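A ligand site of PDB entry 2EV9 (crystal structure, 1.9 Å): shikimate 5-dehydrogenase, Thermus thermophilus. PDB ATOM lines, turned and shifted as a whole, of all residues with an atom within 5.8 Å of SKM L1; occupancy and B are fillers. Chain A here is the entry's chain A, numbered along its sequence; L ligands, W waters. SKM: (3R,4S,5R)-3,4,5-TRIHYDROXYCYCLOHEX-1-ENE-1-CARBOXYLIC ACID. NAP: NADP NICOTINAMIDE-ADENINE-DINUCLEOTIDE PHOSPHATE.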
ATOM      1  N   VAL A   6      30.434  23.126  -5.745  1.00  0.00           N
ATOM      2  CA  VAL A   6      30.160  24.004  -6.875  1.00  0.00           C
ATOM      3  C   VAL A   6      31.419  24.812  -7.186  1.00  0.00           C
ATOM      4  O   VAL A   6      31.956  25.499  -6.320  1.00  0.00           O
ATOM      5  CB  VAL A   6      28.963  24.972  -6.611  1.00  0.00           C
ATOM      6  CG1 VAL A   6      29.192  25.794  -5.347  1.00  0.00           C
ATOM      7  CG2 VAL A   6      28.775  25.880  -7.806  1.00  0.00           C
ATOM      8  N   SER A  14      26.599  31.066  -2.868  1.00  0.00           N
ATOM      9  CA  SER A  14      25.890  30.044  -3.635  1.00  0.00           C
ATOM     10  C   SER A  14      24.865  29.387  -2.721  1.00  0.00           C
ATOM     11  O   SER A  14      25.104  29.196  -1.536  1.00  0.00           O
ATOM     12  CB  SER A  14      26.869  28.995  -4.150  1.00  0.00           C
ATOM     13  OG  SER A  14      26.175  27.948  -4.814  1.00  0.00           O
ATOM     14  N   LEU A  15      23.706  29.037  -3.282  1.00  0.00           N
ATOM     15  CA  LEU A  15      22.651  28.389  -2.500  1.00  0.00           C
ATOM     16  C   LEU A  15      22.694  26.881  -2.697  1.00  0.00           C
ATOM     17  O   LEU A  15      21.902  26.152  -2.110  1.00  0.00           O
ATOM     18  CB  LEU A  15      21.281  28.919  -2.922  1.00  0.00           C
ATOM     19  CG  LEU A  15      21.131  30.434  -2.851  1.00  0.00           C
ATOM     20  CD1 LEU A  15      19.763  30.854  -3.394  1.00  0.00           C
ATOM     21  CD2 LEU A  15      21.309  30.873  -1.408  1.00  0.00           C
ATOM     22  N   SER A  16      23.629  26.430  -3.533  1.00  0.00           N
ATOM     23  CA  SER A  16      23.757  25.001  -3.812  1.00  0.00           C
ATOM     24  C   SER A  16      24.133  24.185  -2.585  1.00  0.00           C
ATOM     25  O   SER A  16      23.539  23.141  -2.325  1.00  0.00           O
ATOM     26  CB  SER A  16      24.780  24.777  -4.937  1.00  0.00           C
ATOM     27  OG  SER A  16      24.189  25.045  -6.209  1.00  0.00           O
ATOM     28  N   PRO A  17      25.136  24.642  -1.801  1.00  0.00           N
ATOM     29  CA  PRO A  17      25.498  23.867  -0.615  1.00  0.00           C
ATOM     30  C   PRO A  17      24.285  23.575   0.263  1.00  0.00           C
ATOM     31  O   PRO A  17      24.110  22.464   0.747  1.00  0.00           O
ATOM     32  CB  PRO A  17      26.540  24.756   0.060  1.00  0.00           C
ATOM     33  CG  PRO A  17      27.242  25.379  -1.115  1.00  0.00           C
ATOM     34  CD  PRO A  17      26.073  25.757  -2.008  1.00  0.00           C
ATOM     35  N   TYR A  33      28.637  18.976   0.342  1.00  0.00           N
ATOM     36  CA  TYR A  33      28.588  19.814  -0.850  1.00  0.00           C
ATOM     37  C   TYR A  33      29.139  21.180  -0.438  1.00  0.00           C
ATOM     38  O   TYR A  33      28.522  21.900   0.331  1.00  0.00           O
ATOM     39  CB  TYR A  33      27.141  19.942  -1.359  1.00  0.00           C
ATOM     40  CG  TYR A  33      27.041  20.579  -2.729  1.00  0.00           C
ATOM     41  CD1 TYR A  33      27.362  21.926  -2.914  1.00  0.00           C
ATOM     42  CD2 TYR A  33      26.654  19.831  -3.846  1.00  0.00           C
ATOM     43  CE1 TYR A  33      27.319  22.511  -4.181  1.00  0.00           C
ATOM     44  CE2 TYR A  33      26.602  20.412  -5.125  1.00  0.00           C
ATOM     45  CZ  TYR A  33      26.939  21.758  -5.275  1.00  0.00           C
ATOM     46  OH  TYR A  33      26.896  22.360  -6.514  1.00  0.00           O
ATOM     47  N   ASN A  58      29.188  20.996  -9.753  1.00  0.00           N
ATOM     48  CA  ASN A  58      28.397  21.898 -10.557  1.00  0.00           C
ATOM     49  C   ASN A  58      29.366  22.992 -10.943  1.00  0.00           C
ATOM     50  O   ASN A  58      30.273  23.325 -10.171  1.00  0.00           O
ATOM     51  CB  ASN A  58      27.254  22.510  -9.747  1.00  0.00           C
ATOM     52  CG  ASN A  58      26.032  21.621  -9.702  1.00  0.00           C
ATOM     53  OD1 ASN A  58      25.468  21.386  -8.632  1.00  0.00           O
ATOM     54  ND2 ASN A  58      25.602  21.123 -10.858  1.00  0.00           N
ATOM     55  N   LEU A  59      29.188  23.545 -12.140  1.00  0.00           N
ATOM     56  CA  LEU A  59      30.049  24.622 -12.599  1.00  0.00           C
ATOM     57  C   LEU A  59      29.184  25.830 -12.882  1.00  0.00           C
ATOM     58  O   LEU A  59      28.102  25.706 -13.472  1.00  0.00           O
ATOM     59  CB  LEU A  59      30.781  24.220 -13.888  1.00  0.00           C
ATOM     60  CG  LEU A  59      31.634  22.960 -13.842  1.00  0.00           C
ATOM     61  CD1 LEU A  59      32.242  22.717 -15.209  1.00  0.00           C
ATOM     62  CD2 LEU A  59      32.708  23.066 -12.761  1.00  0.00           C
ATOM     63  N   THR A  60      29.644  26.995 -12.457  1.00  0.00           N
ATOM     64  CA  THR A  60      28.914  28.236 -12.690  1.00  0.00           C
ATOM     65  C   THR A  60      29.899  29.245 -13.284  1.00  0.00           C
ATOM     66  O   THR A  60      30.999  28.869 -13.684  1.00  0.00           O
ATOM     67  CB  THR A  60      28.322  28.793 -11.385  1.00  0.00           C
ATOM     68  OG1 THR A  60      27.482  29.919 -11.692  1.00  0.00           O
ATOM     69  CG2 THR A  60      29.418  29.218 -10.425  1.00  0.00           C
ATOM     70  N   LEU A  61      29.484  30.507 -13.343  1.00  0.00           N
ATOM     71  CA  LEU A  61      30.343  31.553 -13.877  1.00  0.00           C
ATOM     72  C   LEU A  61      31.686  31.607 -13.170  1.00  0.00           C
ATOM     73  O   LEU A  61      31.740  31.613 -11.941  1.00  0.00           O
ATOM     74  CB  LEU A  61      29.680  32.929 -13.735  1.00  0.00           C
ATOM     75  CG  LEU A  61      28.593  33.288 -14.745  1.00  0.00           C
ATOM     76  CD1 LEU A  61      27.380  32.394 -14.539  1.00  0.00           C
ATOM     77  CD2 LEU A  61      28.231  34.753 -14.555  1.00  0.00           C
ATOM     78  N   LYS A  64      31.534  27.396 -16.890  1.00  0.00           N
ATOM     79  CA  LYS A  64      30.654  26.638 -17.792  1.00  0.00           C
ATOM     80  C   LYS A  64      31.127  26.395 -19.221  1.00  0.00           C
ATOM     81  O   LYS A  64      31.106  25.258 -19.692  1.00  0.00           O
ATOM     82  CB  LYS A  64      29.266  27.290 -17.832  1.00  0.00           C
ATOM     83  CG  LYS A  64      28.506  27.244 -16.516  1.00  0.00           C
ATOM     84  CD  LYS A  64      27.043  27.608 -16.717  1.00  0.00           C
ATOM     85  CE  LYS A  64      26.267  27.514 -15.418  1.00  0.00           C
ATOM     86  NZ  LYS A  64      24.832  27.845 -15.591  1.00  0.00           N
ATOM     87  N   ASN A  85      27.189  22.510 -16.744  1.00  0.00           N
ATOM     88  CA  ASN A  85      26.971  23.011 -15.399  1.00  0.00           C
ATOM     89  C   ASN A  85      27.042  21.850 -14.411  1.00  0.00           C
ATOM     90  O   ASN A  85      26.961  22.057 -13.197  1.00  0.00           O
ATOM     91  CB  ASN A  85      25.584  23.662 -15.283  1.00  0.00           C
ATOM     92  CG  ASN A  85      24.487  22.630 -15.114  1.00  0.00           C
ATOM     93  OD1 ASN A  85      24.480  21.615 -15.811  1.00  0.00           O
ATOM     94  ND2 ASN A  85      23.567  22.872 -14.193  1.00  0.00           N
ATOM     95  N   THR A  86      27.159  20.635 -14.937  1.00  0.00           N
ATOM     96  CA  THR A  86      27.213  19.450 -14.105  1.00  0.00           C
ATOM     97  C   THR A  86      28.243  18.452 -14.592  1.00  0.00           C
ATOM     98  O   THR A  86      28.219  18.019 -15.743  1.00  0.00           O
ATOM     99  CB  THR A  86      25.840  18.745 -14.052  1.00  0.00           C
ATOM    100  OG1 THR A  86      24.879  19.602 -13.440  1.00  0.00           O
ATOM    101  CG2 THR A  86      25.925  17.433 -13.267  1.00  0.00           C
ATOM    102  N   THR A  99      22.187  20.501 -16.854  1.00  0.00           N
ATOM    103  CA  THR A  99      20.896  20.314 -16.223  1.00  0.00           C
ATOM    104  C   THR A  99      20.138  21.640 -16.178  1.00  0.00           C
ATOM    105  O   THR A  99      19.015  21.698 -15.692  1.00  0.00           O
ATOM    106  CB  THR A  99      21.034  19.729 -14.789  1.00  0.00           C
ATOM    107  OG1 THR A  99      21.873  20.587 -13.991  1.00  0.00           O
ATOM    108  CG2 THR A  99      21.662  18.334 -14.850  1.00  0.00           C
ATOM    109  N   ASP A 100      20.758  22.717 -16.674  1.00  0.00           N
ATOM    110  CA  ASP A 100      20.069  24.009 -16.705  1.00  0.00           C
ATOM    111  C   ASP A 100      18.892  23.951 -17.674  1.00  0.00           C
ATOM    112  O   ASP A 100      17.800  24.429 -17.367  1.00  0.00           O
ATOM    113  CB  ASP A 100      21.010  25.146 -17.148  1.00  0.00           C
ATOM    114  CG  ASP A 100      21.960  25.595 -16.058  1.00  0.00           C
ATOM    115  OD1 ASP A 100      21.529  25.702 -14.890  1.00  0.00           O
ATOM    116  OD2 ASP A 100      23.145  25.857 -16.375  1.00  0.00           O
ATOM    117  N   TYR A 207      17.717  35.682  -9.085  1.00  0.00           N
ATOM    118  CA  TYR A 207      16.974  35.517  -7.844  1.00  0.00           C
ATOM    119  C   TYR A 207      17.499  36.371  -6.677  1.00  0.00           C
ATOM    120  O   TYR A 207      17.094  36.196  -5.528  1.00  0.00           O
ATOM    121  CB  TYR A 207      16.905  34.031  -7.462  1.00  0.00           C
ATOM    122  CG  TYR A 207      18.227  33.304  -7.450  1.00  0.00           C
ATOM    123  CD1 TYR A 207      19.067  33.373  -6.337  1.00  0.00           C
ATOM    124  CD2 TYR A 207      18.662  32.579  -8.562  1.00  0.00           C
ATOM    125  CE1 TYR A 207      20.300  32.750  -6.329  1.00  0.00           C
ATOM    126  CE2 TYR A 207      19.902  31.953  -8.566  1.00  0.00           C
ATOM    127  CZ  TYR A 207      20.721  32.042  -7.446  1.00  0.00           C
ATOM    128  OH  TYR A 207      21.962  31.448  -7.444  1.00  0.00           O
ATOM    129  N   LEU A 232      16.719  26.911 -10.320  1.00  0.00           N
ATOM    130  CA  LEU A 232      17.946  26.646  -9.572  1.00  0.00           C
ATOM    131  C   LEU A 232      17.817  25.300  -8.865  1.00  0.00           C
ATOM    132  O   LEU A 232      18.747  24.482  -8.859  1.00  0.00           O
ATOM    133  CB  LEU A 232      18.180  27.754  -8.538  1.00  0.00           C
ATOM    134  CG  LEU A 232      19.357  27.572  -7.575  1.00  0.00           C
ATOM    135  CD1 LEU A 232      20.683  27.603  -8.351  1.00  0.00           C
ATOM    136  CD2 LEU A 232      19.337  28.688  -6.537  1.00  0.00           C
ATOM    137  N   GLN A 235      17.645  22.238 -11.541  1.00  0.00           N
ATOM    138  CA  GLN A 235      18.921  21.927 -12.162  1.00  0.00           C
ATOM    139  C   GLN A 235      19.778  21.202 -11.127  1.00  0.00           C
ATOM    140  O   GLN A 235      20.544  20.302 -11.460  1.00  0.00           O
ATOM    141  CB  GLN A 235      19.617  23.197 -12.676  1.00  0.00           C
ATOM    142  CG  GLN A 235      19.991  24.228 -11.627  1.00  0.00           C
ATOM    143  CD  GLN A 235      21.243  23.848 -10.874  1.00  0.00           C
ATOM    144  OE1 GLN A 235      22.225  23.411 -11.474  1.00  0.00           O
ATOM    145  NE2 GLN A 235      21.212  24.016  -9.556  1.00  0.00           N
HETATM  146  O12 SKM L   1      23.794  25.921 -13.400  1.00  0.00           O
HETATM  147  C8  SKM L   1      23.742  26.294 -12.023  1.00  0.00           C
HETATM  148  C6  SKM L   1      24.879  25.587 -11.218  1.00  0.00           C
HETATM  149  O7  SKM L   1      24.762  24.169 -11.325  1.00  0.00           O
HETATM  150  C5  SKM L   1      24.801  25.985  -9.719  1.00  0.00           C
HETATM  151  C4  SKM L   1      24.645  27.488  -9.544  1.00  0.00           C
HETATM  152  C1  SKM L   1      24.980  28.061  -8.213  1.00  0.00           C
HETATM  153  O2  SKM L   1      25.395  27.261  -7.218  1.00  0.00           O
HETATM  154  O3  SKM L   1      24.872  29.269  -8.005  1.00  0.00           O
HETATM  155  C10 SKM L   1      24.231  28.304 -10.511  1.00  0.00           C
HETATM  156  C9  SKM L   1      23.862  27.842 -11.910  1.00  0.00           C
HETATM  157  O11 SKM L   1      24.867  28.304 -12.824  1.00  0.00           O
HETATM  158  PA  NAP L   2      26.148  36.526 -17.352  1.00  0.00           P
HETATM  159  O1A NAP L   2      25.531  36.475 -16.003  1.00  0.00           O
HETATM  160  O2A NAP L   2      27.507  37.089 -17.550  1.00  0.00           O
HETATM  161  O5B NAP L   2      25.052  37.224 -18.285  1.00  0.00           O
HETATM  162  C5B NAP L   2      25.357  37.477 -19.692  1.00  0.00           C
HETATM  163  C4B NAP L   2      24.162  38.096 -20.370  1.00  0.00           C
HETATM  164  O4B NAP L   2      23.716  39.341 -19.695  1.00  0.00           O
HETATM  165  C3B NAP L   2      24.392  38.453 -21.834  1.00  0.00           C
HETATM  166  O3B NAP L   2      23.216  38.104 -22.585  1.00  0.00           O
HETATM  167  C2B NAP L   2      24.645  39.960 -21.757  1.00  0.00           C
HETATM  168  O2B NAP L   2      24.513  40.658 -22.988  1.00  0.00           O
HETATM  169  C1B NAP L   2      23.626  40.364 -20.729  1.00  0.00           C
HETATM  170  N9A NAP L   2      23.846  41.687 -20.116  1.00  0.00           N
HETATM  171  C8A NAP L   2      24.833  42.054 -19.240  1.00  0.00           C
HETATM  172  N7A NAP L   2      24.772  43.333 -18.859  1.00  0.00           N
HETATM  173  C5A NAP L   2      23.701  43.817 -19.528  1.00  0.00           C
HETATM  174  C6A NAP L   2      23.112  45.122 -19.549  1.00  0.00           C
HETATM  175  N6A NAP L   2      23.586  46.147 -18.842  1.00  0.00           N
HETATM  176  N1A NAP L   2      22.007  45.270 -20.363  1.00  0.00           N
HETATM  177  C2A NAP L   2      21.497  44.242 -21.098  1.00  0.00           C
HETATM  178  N3A NAP L   2      21.988  42.965 -21.128  1.00  0.00           N
HETATM  179  C4A NAP L   2      23.106  42.801 -20.326  1.00  0.00           C
HETATM  180  O3  NAP L   2      26.043  34.999 -17.910  1.00  0.00           O
HETATM  181  PN  NAP L   2      25.037  33.760 -17.819  1.00  0.00           P
HETATM  182  O1N NAP L   2      25.787  32.498 -17.558  1.00  0.00           O
HETATM  183  O2N NAP L   2      24.241  33.821 -19.082  1.00  0.00           O
HETATM  184  O5D NAP L   2      24.004  34.074 -16.595  1.00  0.00           O
HETATM  185  C5D NAP L   2      22.690  34.679 -16.798  1.00  0.00           C
HETATM  186  C4D NAP L   2      22.061  35.241 -15.533  1.00  0.00           C
HETATM  187  O4D NAP L   2      20.982  34.399 -15.029  1.00  0.00           O
HETATM  188  C3D NAP L   2      22.972  35.483 -14.305  1.00  0.00           C
HETATM  189  O3D NAP L   2      22.773  36.733 -13.685  1.00  0.00           O
HETATM  190  C2D NAP L   2      22.736  34.262 -13.422  1.00  0.00           C
HETATM  191  O2D NAP L   2      22.868  34.654 -12.049  1.00  0.00           O
HETATM  192  C1D NAP L   2      21.330  33.817 -13.783  1.00  0.00           C
HETATM  193  N1N NAP L   2      21.140  32.320 -13.879  1.00  0.00           N
HETATM  194  C2N NAP L   2      20.208  31.729 -13.047  1.00  0.00           C
HETATM  195  C3N NAP L   2      19.960  30.360 -13.059  1.00  0.00           C
HETATM  196  C7N NAP L   2      18.921  29.712 -12.139  1.00  0.00           C
HETATM  197  O7N NAP L   2      19.052  28.510 -11.822  1.00  0.00           O
HETATM  198  N7N NAP L   2      17.905  30.501 -11.722  1.00  0.00           N
HETATM  199  C4N NAP L   2      20.706  29.536 -13.980  1.00  0.00           C
HETATM  200  C5N NAP L   2      21.660  30.138 -14.830  1.00  0.00           C
HETATM  201  C6N NAP L   2      21.887  31.511 -14.788  1.00  0.00           C
HETATM  202  P2B NAP L   2      25.787  41.145 -23.901  1.00  0.00           P
HETATM  203  O1X NAP L   2      26.035  40.062 -24.913  1.00  0.00           O
HETATM  204  O2X NAP L   2      25.281  42.453 -24.465  1.00  0.00           O
HETATM  205  O3X NAP L   2      26.947  41.338 -22.947  1.00  0.00           O
HETATM  206  O   HOH W   1      22.503  30.985 -10.930  1.00  0.00           O
HETATM  207  O   HOH W   2      24.993  31.662 -12.750  1.00  0.00           O
HETATM  208  O   HOH W   3      26.475  31.385  -9.690  1.00  0.00           O
HETATM  209  O   HOH W   4      23.031  29.740  -5.816  1.00  0.00           O
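The side-chain hydroxyl (OG) of Ser 14 is in hydrogen-bond range of an oxygen (O2) of SKM L1 (2.6 Å). An oxygen (O7) of SKM L1 is in hydrogen-bond range of the side-chain amide oxygen (OE1) of Gln 235. The side-chain hydroxyl of Ser 16 is in hydrogen-bond range of an oxygen (O2) of SKM L1 (2.7 Å). An oxygen (O12) of SKM L1 is in hydrogen-bond range of the side-chain carboxylate of Asp 100 (2.7 Å). O11 of SKM L1 lies within hydrogen-bond range of NZ of Lys 64, 2.8 Å away. ND2 of Asn 85 lies within hydrogen-bond range of O12 of SKM L1, 3.2 Å away. ND2 of Asn 58 lies within hydrogen-bond range of O7 of SKM L1, at 3.2 Å. O11 of SKM L1 lies within hydrogen-bond range of OG1 of Thr 60 (3.3 Å). The backbone NH of Leu 232 sits close to an oxygen (O7N) of NAP L2.
Residues that only touch SKM L1: Tyr 207 (3.7 Å), Val 6 (3.7 Å) and Leu 59 (3.9 Å). Hydrophobic or aromatic side chains within 4 Å of SKM L1: Val 6.
OG of Ser 14 sits at hydrogen-bond distance from N of Ser 16 (3.2 Å). The side-chain amide oxygen (OE1) of Gln 235 sits at hydrogen-bond distance from the side-chain amide nitrogen (ND2) of Asn 85 (3.1 Å). The side-chain amide nitrogen of Gln 235 lies within hydrogen-bond range of the backbone carbonyl oxygen of Leu 232, at 2.6 Å. The backbone carbonyl oxygen (O) of Asn 85 sits at hydrogen-bond distance from the side-chain amide nitrogen (ND2) of Asn 58, 2.9 Å away. The backbone carbonyl oxygen (O) of Asn 85 lies within hydrogen-bond range of the backbone NH (N) of Leu 59 (2.9 Å). OD1 of Asn 85 lies within hydrogen-bond range of OG1 of Thr 86, 3.1 Å away. The side-chain amide oxygen (OD1) of Asn 85 lies within hydrogen-bond range of the backbone NH (N) of Thr 99 (2.8 Å). ND2 of Asn 58 lies within hydrogen-bond range of OG1 of Thr 86.
Water W4 lies within hydrogen-bond range of OH of Tyr 207, N of Leu 15 and O3 of SKM L1. Water W3 lies within hydrogen-bond range of the side-chain hydroxyl of Thr 60 and an oxygen (O3) of SKM L1. Water W2 lies within hydrogen-bond range of the side-chain hydroxyl (OG1) of Thr 60 (3.2 Å) and an oxygen (O11) of SKM L1 (3.4 Å).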
